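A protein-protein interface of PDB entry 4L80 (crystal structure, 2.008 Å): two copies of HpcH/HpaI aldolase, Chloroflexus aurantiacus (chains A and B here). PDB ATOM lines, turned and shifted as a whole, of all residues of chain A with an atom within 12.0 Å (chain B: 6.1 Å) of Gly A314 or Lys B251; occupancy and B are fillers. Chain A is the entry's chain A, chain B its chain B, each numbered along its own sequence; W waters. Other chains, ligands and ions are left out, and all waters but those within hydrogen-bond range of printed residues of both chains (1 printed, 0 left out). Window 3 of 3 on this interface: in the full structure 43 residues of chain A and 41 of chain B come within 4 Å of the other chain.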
ATOM      1  N   PHE A 295      14.747 -14.181 -12.648  1.00  0.00           N
ATOM      2  CA  PHE A 295      16.003 -14.699 -13.175  1.00  0.00           C
ATOM      3  C   PHE A 295      16.850 -15.260 -12.039  1.00  0.00           C
ATOM      4  O   PHE A 295      17.557 -16.255 -12.211  1.00  0.00           O
ATOM      5  CB  PHE A 295      16.769 -13.619 -13.939  1.00  0.00           C
ATOM      6  CG  PHE A 295      17.946 -14.147 -14.712  1.00  0.00           C
ATOM      7  CD1 PHE A 295      19.229 -14.064 -14.194  1.00  0.00           C
ATOM      8  CD2 PHE A 295      17.767 -14.734 -15.954  1.00  0.00           C
ATOM      9  CE1 PHE A 295      20.312 -14.553 -14.905  1.00  0.00           C
ATOM     10  CE2 PHE A 295      18.846 -15.224 -16.669  1.00  0.00           C
ATOM     11  CZ  PHE A 295      20.119 -15.133 -16.144  1.00  0.00           C
ATOM     12  N   ARG A 298      15.733 -18.677 -11.338  1.00  0.00           N
ATOM     13  CA  ARG A 298      16.243 -19.582 -12.364  1.00  0.00           C
ATOM     14  C   ARG A 298      17.677 -20.007 -12.052  1.00  0.00           C
ATOM     15  O   ARG A 298      18.058 -21.154 -12.290  1.00  0.00           O
ATOM     16  CB  ARG A 298      16.167 -18.935 -13.750  1.00  0.00           C
ATOM     17  CG  ARG A 298      14.748 -18.679 -14.249  1.00  0.00           C
ATOM     18  CD  ARG A 298      14.750 -18.063 -15.645  1.00  0.00           C
ATOM     19  NE  ARG A 298      15.245 -18.991 -16.661  1.00  0.00           N
ATOM     20  CZ  ARG A 298      15.552 -18.644 -17.908  1.00  0.00           C
ATOM     21  NH1 ARG A 298      15.423 -17.382 -18.300  1.00  0.00           N
ATOM     22  NH2 ARG A 298      15.994 -19.554 -18.763  1.00  0.00           N
ATOM     23  N   ILE A 299      18.464 -19.078 -11.515  1.00  0.00           N
ATOM     24  CA  ILE A 299      19.835 -19.370 -11.108  1.00  0.00           C
ATOM     25  C   ILE A 299      19.857 -20.360  -9.948  1.00  0.00           C
ATOM     26  O   ILE A 299      20.583 -21.354  -9.985  1.00  0.00           O
ATOM     27  CB  ILE A 299      20.595 -18.089 -10.698  1.00  0.00           C
ATOM     28  CG1 ILE A 299      20.760 -17.157 -11.899  1.00  0.00           C
ATOM     29  CG2 ILE A 299      21.956 -18.435 -10.111  1.00  0.00           C
ATOM     30  CD1 ILE A 299      21.363 -15.815 -11.550  1.00  0.00           C
ATOM     31  N   ALA A 302      18.902 -23.781 -11.150  1.00  0.00           N
ATOM     32  CA  ALA A 302      19.886 -24.412 -12.028  1.00  0.00           C
ATOM     33  C   ALA A 302      20.924 -25.229 -11.257  1.00  0.00           C
ATOM     34  O   ALA A 302      21.489 -26.187 -11.786  1.00  0.00           O
ATOM     35  CB  ALA A 302      20.573 -23.364 -12.898  1.00  0.00           C
ATOM     36  N   VAL A 309      28.784 -25.055 -11.897  1.00  0.00           N
ATOM     37  CA  VAL A 309      28.722 -24.103 -12.999  1.00  0.00           C
ATOM     38  C   VAL A 309      27.514 -24.404 -13.890  1.00  0.00           C
ATOM     39  O   VAL A 309      27.104 -25.558 -14.019  1.00  0.00           O
ATOM     40  CB  VAL A 309      30.033 -24.131 -13.831  1.00  0.00           C
ATOM     41  CG1 VAL A 309      30.206 -25.476 -14.528  1.00  0.00           C
ATOM     42  CG2 VAL A 309      30.073 -22.982 -14.836  1.00  0.00           C
ATOM     43  N   ALA A 310      26.938 -23.363 -14.484  1.00  0.00           N
ATOM     44  CA  ALA A 310      25.789 -23.519 -15.372  1.00  0.00           C
ATOM     45  C   ALA A 310      25.672 -22.347 -16.342  1.00  0.00           C
ATOM     46  O   ALA A 310      26.128 -21.242 -16.047  1.00  0.00           O
ATOM     47  CB  ALA A 310      24.511 -23.663 -14.561  1.00  0.00           C
ATOM     48  N   MET A 311      25.061 -22.595 -17.498  1.00  0.00           N
ATOM     49  CA  MET A 311      24.832 -21.550 -18.494  1.00  0.00           C
ATOM     50  C   MET A 311      23.345 -21.235 -18.626  1.00  0.00           C
ATOM     51  O   MET A 311      22.531 -22.131 -18.847  1.00  0.00           O
ATOM     52  CB  MET A 311      25.392 -21.970 -19.859  1.00  0.00           C
ATOM     53  CG  MET A 311      26.908 -22.090 -19.919  1.00  0.00           C
ATOM     54  SD  MET A 311      27.763 -20.499 -19.900  1.00  0.00           S
ATOM     55  CE  MET A 311      27.113 -19.733 -21.384  1.00  0.00           C
ATOM     56  N   ILE A 312      22.993 -19.960 -18.485  1.00  0.00           N
ATOM     57  CA  ILE A 312      21.609 -19.522 -18.646  1.00  0.00           C
ATOM     58  C   ILE A 312      21.525 -18.321 -19.587  1.00  0.00           C
ATOM     59  O   ILE A 312      22.051 -17.248 -19.284  1.00  0.00           O
ATOM     60  CB  ILE A 312      20.955 -19.159 -17.295  1.00  0.00           C
ATOM     61  CG1 ILE A 312      20.895 -20.383 -16.379  1.00  0.00           C
ATOM     62  CG2 ILE A 312      19.560 -18.597 -17.514  1.00  0.00           C
ATOM     63  CD1 ILE A 312      20.186 -20.129 -15.066  1.00  0.00           C
ATOM     64  N   ASP A 313      20.864 -18.517 -20.727  1.00  0.00           N
ATOM     65  CA  ASP A 313      20.707 -17.475 -21.744  1.00  0.00           C
ATOM     66  C   ASP A 313      22.039 -16.849 -22.171  1.00  0.00           C
ATOM     67  O   ASP A 313      22.122 -15.643 -22.406  1.00  0.00           O
ATOM     68  CB  ASP A 313      19.734 -16.389 -21.269  1.00  0.00           C
ATOM     69  CG  ASP A 313      18.304 -16.891 -21.165  1.00  0.00           C
ATOM     70  OD1 ASP A 313      17.934 -17.800 -21.937  1.00  0.00           O
ATOM     71  OD2 ASP A 313      17.549 -16.372 -20.314  1.00  0.00           O
ATOM     72  N   GLY A 314      23.076 -17.676 -22.268  1.00  0.00           N
ATOM     73  CA  GLY A 314      24.390 -17.204 -22.670  1.00  0.00           C
ATOM     74  C   GLY A 314      25.211 -16.661 -21.514  1.00  0.00           C
ATOM     75  O   GLY A 314      26.415 -16.431 -21.649  1.00  0.00           O
ATOM     76  N   LYS A 315      24.557 -16.450 -20.375  1.00  0.00           N
ATOM     77  CA  LYS A 315      25.232 -15.953 -19.182  1.00  0.00           C
ATOM     78  C   LYS A 315      25.689 -17.109 -18.297  1.00  0.00           C
ATOM     79  O   LYS A 315      24.898 -17.988 -17.947  1.00  0.00           O
ATOM     80  CB  LYS A 315      24.312 -15.016 -18.396  1.00  0.00           C
ATOM     81  CG  LYS A 315      23.850 -13.797 -19.181  1.00  0.00           C
ATOM     82  CD  LYS A 315      22.817 -13.002 -18.401  1.00  0.00           C
ATOM     83  CE  LYS A 315      23.395 -12.466 -17.099  1.00  0.00           C
ATOM     84  NZ  LYS A 315      24.390 -11.377 -17.329  1.00  0.00           N
ATOM     85  N   MET A 316      26.969 -17.105 -17.941  1.00  0.00           N
ATOM     86  CA  MET A 316      27.537 -18.160 -17.112  1.00  0.00           C
ATOM     87  C   MET A 316      27.178 -17.967 -15.639  1.00  0.00           C
ATOM     88  O   MET A 316      27.167 -16.842 -15.134  1.00  0.00           O
ATOM     89  CB  MET A 316      29.055 -18.212 -17.284  1.00  0.00           C
ATOM     90  CG  MET A 316      29.728 -19.341 -16.522  1.00  0.00           C
ATOM     91  SD  MET A 316      31.522 -19.295 -16.680  1.00  0.00           S
ATOM     92  CE  MET A 316      31.714 -19.526 -18.446  1.00  0.00           C
ATOM     93  N   GLN A 317      26.883 -19.068 -14.957  1.00  0.00           N
ATOM     94  CA  GLN A 317      26.530 -19.019 -13.544  1.00  0.00           C
ATOM     95  C   GLN A 317      27.454 -19.918 -12.728  1.00  0.00           C
ATOM     96  O   GLN A 317      27.962 -20.918 -13.232  1.00  0.00           O
ATOM     97  CB  GLN A 317      25.075 -19.455 -13.346  1.00  0.00           C
ATOM     98  CG  GLN A 317      24.085 -18.848 -14.333  1.00  0.00           C
ATOM     99  CD  GLN A 317      23.893 -17.358 -14.132  1.00  0.00           C
ATOM    100  OE1 GLN A 317      24.182 -16.823 -13.062  1.00  0.00           O
ATOM    101  NE2 GLN A 317      23.405 -16.679 -15.165  1.00  0.00           N
ATOM    102  N   ASP A 318      27.675 -19.549 -11.471  1.00  0.00           N
ATOM    103  CA  ASP A 318      28.420 -20.390 -10.535  1.00  0.00           C
ATOM    104  C   ASP A 318      28.069 -20.048  -9.087  1.00  0.00           C
ATOM    105  O   ASP A 318      27.084 -19.348  -8.838  1.00  0.00           O
ATOM    106  CB  ASP A 318      29.932 -20.312 -10.775  1.00  0.00           C
ATOM    107  CG  ASP A 318      30.436 -18.890 -10.894  1.00  0.00           C
ATOM    108  OD1 ASP A 318      29.905 -17.993 -10.201  1.00  0.00           O
ATOM    109  OD2 ASP A 318      31.374 -18.675 -11.689  1.00  0.00           O
ATOM    110  N   THR A 321      27.258 -16.254  -8.383  1.00  0.00           N
ATOM    111  CA  THR A 321      25.996 -15.746  -8.923  1.00  0.00           C
ATOM    112  C   THR A 321      24.818 -16.353  -8.167  1.00  0.00           C
ATOM    113  O   THR A 321      23.748 -15.752  -8.073  1.00  0.00           O
ATOM    114  CB  THR A 321      25.849 -16.022 -10.435  1.00  0.00           C
ATOM    115  OG1 THR A 321      25.744 -17.432 -10.667  1.00  0.00           O
ATOM    116  CG2 THR A 321      27.040 -15.477 -11.195  1.00  0.00           C
ATOM    117  N   GLY B 248      30.699 -12.408 -17.066  1.00  0.00           N
ATOM    118  CA  GLY B 248      29.817 -13.563 -17.067  1.00  0.00           C
ATOM    119  C   GLY B 248      29.035 -13.827 -18.341  1.00  0.00           C
ATOM    120  O   GLY B 248      28.817 -14.981 -18.706  1.00  0.00           O
ATOM    121  N   ASP B 249      28.600 -12.765 -19.013  1.00  0.00           N
ATOM    122  CA  ASP B 249      27.840 -12.920 -20.247  1.00  0.00           C
ATOM    123  C   ASP B 249      28.770 -13.299 -21.399  1.00  0.00           C
ATOM    124  O   ASP B 249      29.288 -12.434 -22.109  1.00  0.00           O
ATOM    125  CB  ASP B 249      27.065 -11.642 -20.571  1.00  0.00           C
ATOM    126  CG  ASP B 249      25.933 -11.881 -21.553  1.00  0.00           C
ATOM    127  OD1 ASP B 249      26.008 -12.859 -22.324  1.00  0.00           O
ATOM    128  OD2 ASP B 249      24.967 -11.090 -21.553  1.00  0.00           O
ATOM    129  N   ILE B 250      28.969 -14.601 -21.573  1.00  0.00           N
ATOM    130  CA  ILE B 250      29.901 -15.133 -22.561  1.00  0.00           C
ATOM    131  C   ILE B 250      29.512 -14.774 -23.994  1.00  0.00           C
ATOM    132  O   ILE B 250      30.370 -14.470 -24.827  1.00  0.00           O
ATOM    133  CB  ILE B 250      30.009 -16.665 -22.436  1.00  0.00           C
ATOM    134  CG1 ILE B 250      30.314 -17.056 -20.988  1.00  0.00           C
ATOM    135  CG2 ILE B 250      31.070 -17.214 -23.378  1.00  0.00           C
ATOM    136  CD1 ILE B 250      31.603 -16.470 -20.458  1.00  0.00           C
ATOM    137  N   LYS B 251      28.213 -14.795 -24.271  1.00  0.00           N
ATOM    138  CA  LYS B 251      27.710 -14.578 -25.625  1.00  0.00           C
ATOM    139  C   LYS B 251      27.735 -13.108 -26.040  1.00  0.00           C
ATOM    140  O   LYS B 251      27.918 -12.792 -27.217  1.00  0.00           O
ATOM    141  CB  LYS B 251      26.295 -15.152 -25.770  1.00  0.00           C
ATOM    142  CG  LYS B 251      26.245 -16.574 -26.323  1.00  0.00           C
ATOM    143  CD  LYS B 251      27.229 -17.487 -25.605  1.00  0.00           C
ATOM    144  CE  LYS B 251      27.128 -18.932 -26.069  1.00  0.00           C
ATOM    145  NZ  LYS B 251      28.270 -19.737 -25.546  1.00  0.00           N
ATOM    146  N   ASP B 252      27.551 -12.209 -25.079  1.00  0.00           N
ATOM    147  CA  ASP B 252      27.576 -10.782 -25.373  1.00  0.00           C
ATOM    148  C   ASP B 252      29.019 -10.283 -25.454  1.00  0.00           C
ATOM    149  O   ASP B 252      29.545  -9.704 -24.501  1.00  0.00           O
ATOM    150  CB  ASP B 252      26.792 -10.001 -24.316  1.00  0.00           C
ATOM    151  CG  ASP B 252      26.465  -8.591 -24.759  1.00  0.00           C
ATOM    152  OD1 ASP B 252      27.025  -8.140 -25.777  1.00  0.00           O
ATOM    153  OD2 ASP B 252      25.653  -7.925 -24.083  1.00  0.00           O
ATOM    154  N   GLU B 253      29.650 -10.505 -26.602  1.00  0.00           N
ATOM    155  CA  GLU B 253      31.056 -10.158 -26.788  1.00  0.00           C
ATOM    156  C   GLU B 253      31.286  -8.652 -26.871  1.00  0.00           C
ATOM    157  O   GLU B 253      32.359  -8.162 -26.525  1.00  0.00           O
ATOM    158  CB  GLU B 253      31.622 -10.846 -28.034  1.00  0.00           C
ATOM    159  CG  GLU B 253      31.634 -12.363 -27.945  1.00  0.00           C
ATOM    160  CD  GLU B 253      32.384 -13.010 -29.094  1.00  0.00           C
ATOM    161  OE1 GLU B 253      32.989 -12.276 -29.901  1.00  0.00           O
ATOM    162  OE2 GLU B 253      32.374 -14.256 -29.186  1.00  0.00           O
ATOM    163  N   ALA B 254      30.278  -7.922 -27.335  1.00  0.00           N
ATOM    164  CA  ALA B 254      30.375  -6.470 -27.428  1.00  0.00           C
ATOM    165  C   ALA B 254      30.459  -5.850 -26.037  1.00  0.00           C
ATOM    166  O   ALA B 254      31.241  -4.927 -25.807  1.00  0.00           O
ATOM    167  CB  ALA B 254      29.191  -5.902 -28.198  1.00  0.00           C
ATOM    168  N   ASN B 277      36.138 -18.051 -26.788  1.00  0.00           N
ATOM    169  CA  ASN B 277      35.751 -16.842 -27.512  1.00  0.00           C
ATOM    170  C   ASN B 277      36.237 -15.558 -26.842  1.00  0.00           C
ATOM    171  O   ASN B 277      36.425 -14.539 -27.507  1.00  0.00           O
ATOM    172  CB  ASN B 277      34.237 -16.790 -27.751  1.00  0.00           C
ATOM    173  CG  ASN B 277      33.445 -16.560 -26.475  1.00  0.00           C
ATOM    174  OD1 ASN B 277      33.684 -17.205 -25.454  1.00  0.00           O
ATOM    175  ND2 ASN B 277      32.497 -15.632 -26.531  1.00  0.00           N
HETATM  176  O   HOH W   1      23.859 -13.279 -23.539  1.00  0.00           O
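Of the 15 printed residues of chain A, 3 touch a printed residue of chain B.
Printed residues of chain A that touch a printed residue of chain B: Gly A314, Lys A315 and Met A316.
Along chain A the printed residues that touch a printed residue of chain B span positions 314 to 316.
Of the 8 printed residues of chain B, 4 touch a printed residue of chain A.
Among the printed residues, 7 pairs touch across the chains.
No position is printed for both chains.
Of the 7 pairs that touch across the chains among the printed residues, none has its exchanged pair printed and touching as well.
The backbone NH of Ile B250 lies within hydrogen-bond range of the backbone carbonyl oxygen of Gly A314.
The backbone carbonyl oxygen (O) of Gly B248 is in hydrogen-bond range of the backbone NH (N) of Met A316, 2.9 Å away.
Among the printed residues, pairs that only touch across the chains: Gly A314 with Lys B251 (3.6 Å), Gly A314 with Asp B249 (3.7 Å), Met A316 with Ile B250 (3.7 Å), Lys A315 with Asp B249 (3.7 Å) and Lys A315 with Gly B248 (3.7 Å).
The side-chain amide nitrogen (NE2) of Gln A317 sits at hydrogen-bond distance from the backbone carbonyl oxygen (O) of Lys A315 (3.4 Å).
OD1 of Asp B249 lies within hydrogen-bond range of N of Asp B252 (3.2 Å).
The backbone carbonyl oxygen (O) of Ile B250 lies within hydrogen-bond range of the side-chain amide nitrogen (ND2) of Asn B277, at 3.0 Å.
Ala A302 touches none of the printed residues of chain B.
Gly A314 touches just these residues of chain B: Asp B249 (3.7 Å), Ile B250 (3.1 Å) and Lys B251 (3.6 Å).
Printed residues of chain B within 4 Å of Lys A315: Gly B248 (3.7 Å) and Asp B249 (3.7 Å).
Printed residues of chain B within 4 Å of Met A316: Gly B248 (2.9 Å) and Ile B250 (3.7 Å).
Ile B250 touches two residues of chain A.
Lys B251 touches just one residue of chain A: Gly A314.
No residue of chain A comes within 4 Å of Glu B253.
Water W1 bridges the side-chain carboxylate (OD1) of Asp B249 (2.5 Å) and the backbone carbonyl oxygen (O) of Asp A313 (3.1 Å).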
